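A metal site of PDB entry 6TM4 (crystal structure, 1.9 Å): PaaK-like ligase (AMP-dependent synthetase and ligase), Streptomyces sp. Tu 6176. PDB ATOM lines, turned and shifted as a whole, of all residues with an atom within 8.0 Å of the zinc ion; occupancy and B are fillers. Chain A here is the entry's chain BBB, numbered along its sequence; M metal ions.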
ATOM      1  N   GLY A 247      -6.092  17.711  -2.804  1.00  0.00           N
ATOM      2  CA  GLY A 247      -4.942  17.659  -3.714  1.00  0.00           C
ATOM      3  C   GLY A 247      -5.315  18.252  -5.047  1.00  0.00           C
ATOM      4  O   GLY A 247      -6.490  18.159  -5.442  1.00  0.00           O
ATOM      5  N   GLN A 248      -4.320  18.812  -5.713  1.00  0.00           N
ATOM      6  CA  GLN A 248      -4.465  19.538  -6.992  1.00  0.00           C
ATOM      7  C   GLN A 248      -4.851  18.544  -8.091  1.00  0.00           C
ATOM      8  O   GLN A 248      -4.356  17.383  -8.072  1.00  0.00           O
ATOM      9  CB  GLN A 248      -3.164  20.275  -7.289  1.00  0.00           C
ATOM     10  CG  GLN A 248      -3.263  21.281  -8.423  1.00  0.00           C
ATOM     11  CD  GLN A 248      -1.885  21.788  -8.811  1.00  0.00           C
ATOM     12  OE1 GLN A 248      -1.192  21.179  -9.631  1.00  0.00           O
ATOM     13  NE2 GLN A 248      -1.463  22.858  -8.146  1.00  0.00           N
ATOM     14  N   CYS A 249      -5.721  18.977  -9.010  1.00  0.00           N
ATOM     15  CA  CYS A 249      -6.003  18.294 -10.294  1.00  0.00           C
ATOM     16  C   CYS A 249      -5.138  18.916 -11.392  1.00  0.00           C
ATOM     17  O   CYS A 249      -4.539  19.975 -11.178  1.00  0.00           O
ATOM     18  CB  CYS A 249      -7.485  18.409 -10.624  1.00  0.00           C
ATOM     19  SG  CYS A 249      -7.942  20.093 -11.146  1.00  0.00           S
ATOM     20  N   PRO A 250      -5.084  18.345 -12.611  1.00  0.00           N
ATOM     21  CA  PRO A 250      -4.303  18.944 -13.696  1.00  0.00           C
ATOM     22  C   PRO A 250      -4.755  20.365 -14.086  1.00  0.00           C
ATOM     23  O   PRO A 250      -4.001  21.029 -14.752  1.00  0.00           O
ATOM     24  CB  PRO A 250      -4.508  17.979 -14.872  1.00  0.00           C
ATOM     25  CG  PRO A 250      -4.909  16.667 -14.226  1.00  0.00           C
ATOM     26  CD  PRO A 250      -5.724  17.084 -13.021  1.00  0.00           C
ATOM     27  N   GLU A 251      -5.948  20.799 -13.671  1.00  0.00           N
ATOM     28  CA  GLU A 251      -6.482  22.149 -13.996  1.00  0.00           C
ATOM     29  C   GLU A 251      -6.045  23.184 -12.956  1.00  0.00           C
ATOM     30  O   GLU A 251      -6.310  24.382 -13.170  1.00  0.00           O
ATOM     31  CB  GLU A 251      -8.002  22.072 -14.128  1.00  0.00           C
ATOM     32  CG  GLU A 251      -8.418  21.389 -15.420  1.00  0.00           C
ATOM     33  CD  GLU A 251      -8.326  22.359 -16.575  1.00  0.00           C
ATOM     34  OE1 GLU A 251      -7.204  22.586 -17.080  1.00  0.00           O
ATOM     35  OE2 GLU A 251      -9.363  22.965 -16.895  1.00  0.00           O
ATOM     36  N   GLY A 252      -5.410  22.760 -11.866  1.00  0.00           N
ATOM     37  CA  GLY A 252      -4.803  23.651 -10.868  1.00  0.00           C
ATOM     38  C   GLY A 252      -5.700  23.946  -9.689  1.00  0.00           C
ATOM     39  O   GLY A 252      -5.283  24.784  -8.877  1.00  0.00           O
ATOM     40  N   ARG A 253      -6.852  23.282  -9.551  1.00  0.00           N
ATOM     41  CA  ARG A 253      -7.729  23.352  -8.348  1.00  0.00           C
ATOM     42  C   ARG A 253      -7.388  22.209  -7.381  1.00  0.00           C
ATOM     43  O   ARG A 253      -7.024  21.101  -7.834  1.00  0.00           O
ATOM     44  CB  ARG A 253      -9.203  23.314  -8.734  1.00  0.00           C
ATOM     45  CG  ARG A 253      -9.596  24.355  -9.775  1.00  0.00           C
ATOM     46  CD  ARG A 253      -9.272  25.793  -9.365  1.00  0.00           C
ATOM     47  NE  ARG A 253      -9.497  26.037  -7.936  1.00  0.00           N
ATOM     48  CZ  ARG A 253     -10.701  26.123  -7.343  1.00  0.00           C
ATOM     49  NH1 ARG A 253     -11.810  26.003  -8.036  1.00  0.00           N
ATOM     50  NH2 ARG A 253     -10.781  26.313  -6.033  1.00  0.00           N
ATOM     51  N   MET A 254      -7.541  22.457  -6.089  1.00  0.00           N
ATOM     52  CA  MET A 254      -7.469  21.412  -5.048  1.00  0.00           C
ATOM     53  C   MET A 254      -8.862  20.809  -4.894  1.00  0.00           C
ATOM     54  O   MET A 254      -9.843  21.561  -4.738  1.00  0.00           O
ATOM     55  CB  MET A 254      -6.949  21.948  -3.705  1.00  0.00           C
ATOM     56  CG  MET A 254      -5.509  22.388  -3.805  1.00  0.00           C
ATOM     57  SD  MET A 254      -4.712  22.614  -2.197  1.00  0.00           S
ATOM     58  CE  MET A 254      -5.526  24.121  -1.674  1.00  0.00           C
ATOM     59  N   HIS A 255      -8.940  19.478  -4.928  1.00  0.00           N
ATOM     60  CA  HIS A 255     -10.205  18.716  -4.720  1.00  0.00           C
ATOM     61  C   HIS A 255     -10.141  18.001  -3.371  1.00  0.00           C
ATOM     62  O   HIS A 255      -9.116  17.434  -3.059  1.00  0.00           O
ATOM     63  CB  HIS A 255     -10.402  17.735  -5.893  1.00  0.00           C
ATOM     64  CG  HIS A 255     -10.862  18.376  -7.156  1.00  0.00           C
ATOM     65  ND1 HIS A 255     -12.193  18.412  -7.484  1.00  0.00           N
ATOM     66  CD2 HIS A 255     -10.207  18.975  -8.177  1.00  0.00           C
ATOM     67  CE1 HIS A 255     -12.352  19.007  -8.651  1.00  0.00           C
ATOM     68  NE2 HIS A 255     -11.149  19.373  -9.111  1.00  0.00           N
ATOM     69  N   ASP A 307     -19.201  22.848  -7.763  1.00  0.00           N
ATOM     70  CA  ASP A 307     -19.236  23.172  -9.214  1.00  0.00           C
ATOM     71  C   ASP A 307     -18.253  22.259  -9.936  1.00  0.00           C
ATOM     72  O   ASP A 307     -17.149  22.041  -9.449  1.00  0.00           O
ATOM     73  CB  ASP A 307     -18.918  24.650  -9.476  1.00  0.00           C
ATOM     74  CG  ASP A 307     -19.997  25.629  -8.962  1.00  0.00           C
ATOM     75  OD1 ASP A 307     -21.155  25.157  -8.682  1.00  0.00           O
ATOM     76  OD2 ASP A 307     -19.691  26.835  -8.895  1.00  0.00           O
ATOM     77  N   PRO A 308     -18.601  21.688 -11.113  1.00  0.00           N
ATOM     78  CA  PRO A 308     -17.668  20.847 -11.842  1.00  0.00           C
ATOM     79  C   PRO A 308     -16.383  21.603 -12.201  1.00  0.00           C
ATOM     80  O   PRO A 308     -16.388  22.815 -12.403  1.00  0.00           O
ATOM     81  CB  PRO A 308     -18.421  20.443 -13.133  1.00  0.00           C
ATOM     82  CG  PRO A 308     -19.583  21.401 -13.229  1.00  0.00           C
ATOM     83  CD  PRO A 308     -19.889  21.814 -11.798  1.00  0.00           C
ATOM     84  N   CYS A 309     -15.289  20.819 -12.220  1.00  0.00           N
ATOM     85  CA  CYS A 309     -13.969  21.252 -12.723  1.00  0.00           C
ATOM     86  C   CYS A 309     -13.721  20.558 -14.104  1.00  0.00           C
ATOM     87  O   CYS A 309     -14.143  19.376 -14.241  1.00  0.00           O
ATOM     88  CB  CYS A 309     -12.883  20.885 -11.715  1.00  0.00           C
ATOM     89  SG  CYS A 309     -11.306  21.720 -12.060  1.00  0.00           S
ATOM     90  N   GLY A 310     -12.913  21.263 -14.937  1.00  0.00           N
ATOM     91  CA  GLY A 310     -12.360  20.739 -16.215  1.00  0.00           C
ATOM     92  C   GLY A 310     -11.694  19.373 -16.081  1.00  0.00           C
ATOM     93  O   GLY A 310     -11.723  18.641 -17.059  1.00  0.00           O
ATOM     94  N   CYS A 311     -11.115  19.026 -14.928  1.00  0.00           N
ATOM     95  CA  CYS A 311     -10.425  17.712 -14.697  1.00  0.00           C
ATOM     96  C   CYS A 311     -11.400  16.529 -14.799  1.00  0.00           C
ATOM     97  O   CYS A 311     -10.924  15.432 -15.132  1.00  0.00           O
ATOM     98  CB  CYS A 311      -9.711  17.641 -13.353  1.00  0.00           C
ATOM     99  SG  CYS A 311     -10.796  17.747 -11.891  1.00  0.00           S
ATOM    100  N   GLY A 312     -12.690  16.719 -14.480  1.00  0.00           N
ATOM    101  CA  GLY A 312     -13.704  15.625 -14.464  1.00  0.00           C
ATOM    102  C   GLY A 312     -13.722  14.780 -13.182  1.00  0.00           C
ATOM    103  O   GLY A 312     -14.537  13.860 -13.092  1.00  0.00           O
ATOM    104  N   TRP A 313     -12.884  15.055 -12.190  1.00  0.00           N
ATOM    105  CA  TRP A 313     -12.963  14.350 -10.879  1.00  0.00           C
ATOM    106  C   TRP A 313     -14.288  14.700 -10.202  1.00  0.00           C
ATOM    107  O   TRP A 313     -14.638  15.928 -10.141  1.00  0.00           O
ATOM    108  CB  TRP A 313     -11.829  14.755  -9.955  1.00  0.00           C
ATOM    109  CG  TRP A 313     -10.452  14.449 -10.452  1.00  0.00           C
ATOM    110  CD1 TRP A 313     -10.096  13.812 -11.607  1.00  0.00           C
ATOM    111  CD2 TRP A 313      -9.247  14.760  -9.754  1.00  0.00           C
ATOM    112  NE1 TRP A 313      -8.735  13.737 -11.682  1.00  0.00           N
ATOM    113  CE2 TRP A 313      -8.182  14.292 -10.559  1.00  0.00           C
ATOM    114  CE3 TRP A 313      -8.965  15.383  -8.538  1.00  0.00           C
ATOM    115  CZ2 TRP A 313      -6.850  14.429 -10.165  1.00  0.00           C
ATOM    116  CZ3 TRP A 313      -7.651  15.526  -8.166  1.00  0.00           C
ATOM    117  CH2 TRP A 313      -6.608  15.047  -8.969  1.00  0.00           C
ATOM    118  N   LEU A 314     -14.986  13.686  -9.704  1.00  0.00           N
ATOM    119  CA  LEU A 314     -16.338  13.878  -9.082  1.00  0.00           C
ATOM    120  C   LEU A 314     -16.137  14.176  -7.584  1.00  0.00           C
ATOM    121  O   LEU A 314     -16.553  13.383  -6.739  1.00  0.00           O
ATOM    122  CB  LEU A 314     -17.195  12.650  -9.384  1.00  0.00           C
ATOM    123  CG  LEU A 314     -17.561  12.410 -10.852  1.00  0.00           C
ATOM    124  CD1 LEU A 314     -18.379  11.137 -10.986  1.00  0.00           C
ATOM    125  CD2 LEU A 314     -18.324  13.594 -11.461  1.00  0.00           C
ATOM    126  N   LEU A 315     -15.500  15.312  -7.292  1.00  0.00           N
ATOM    127  CA  LEU A 315     -15.136  15.794  -5.938  1.00  0.00           C
ATOM    128  C   LEU A 315     -15.217  17.345  -5.906  1.00  0.00           C
ATOM    129  O   LEU A 315     -14.679  18.015  -6.761  1.00  0.00           O
ATOM    130  CB  LEU A 315     -13.708  15.350  -5.614  1.00  0.00           C
ATOM    131  CG  LEU A 315     -13.506  13.861  -5.364  1.00  0.00           C
ATOM    132  CD1 LEU A 315     -12.015  13.554  -5.283  1.00  0.00           C
ATOM    133  CD2 LEU A 315     -14.244  13.401  -4.097  1.00  0.00           C
ATOM    134  N   PRO A 316     -15.706  17.890  -4.755  1.00  0.00           N
ATOM    135  CA  PRO A 316     -15.709  19.338  -4.521  1.00  0.00           C
ATOM    136  C   PRO A 316     -14.283  19.895  -4.529  1.00  0.00           C
ATOM    137  O   PRO A 316     -13.318  19.182  -4.187  1.00  0.00           O
ATOM    138  CB  PRO A 316     -16.275  19.518  -3.101  1.00  0.00           C
ATOM    139  CG  PRO A 316     -16.960  18.211  -2.774  1.00  0.00           C
ATOM    140  CD  PRO A 316     -16.198  17.159  -3.570  1.00  0.00           C
ATOM    141  N   THR A 317     -14.177  21.162  -4.914  1.00  0.00           N
ATOM    142  CA  THR A 317     -12.928  21.957  -4.891  1.00  0.00           C
ATOM    143  C   THR A 317     -12.898  22.772  -3.606  1.00  0.00           C
ATOM    144  O   THR A 317     -13.957  23.034  -3.012  1.00  0.00           O
ATOM    145  CB  THR A 317     -12.849  22.886  -6.110  1.00  0.00           C
ATOM    146  OG1 THR A 317     -13.962  23.774  -6.026  1.00  0.00           O
ATOM    147  CG2 THR A 317     -12.852  22.120  -7.420  1.00  0.00           C
HETATM  148 ZN    ZN M   1     -10.189  19.760 -10.962  1.00  0.00          ZN
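Within 4 Å of the zinc ion: Cys 249, His 255, Cys 309 and Cys 311.
The zinc ion is bound by a ring nitrogen (NE2) of His 255 (2.1 Å), the side-chain sulfur (SG) of Cys 249 (2.3 Å), the side-chain sulfur (SG) of Cys 311 (2.3 Å) and the side-chain sulfur (SG) of Cys 309 (2.5 Å).
The side-chain sulfur (SG) of Cys 311 lies close to the backbone NH (N) of Trp 313.
SG of Cys 249 sits close to N of Glu 251.
N of Gly 252 lies close to SG of Cys 249 (3.7 Å).
The backbone carbonyl oxygen (O) of Gly 247 sits at hydrogen-bond distance from the backbone NH (N) of His 255 (2.8 Å).
A ring nitrogen (ND1) of His 255 is in hydrogen-bond range of the backbone carbonyl oxygen (O) of Leu 315, 2.6 Å away.
SG of Cys 249 sits close to O of Arg 253 (3.6 Å).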
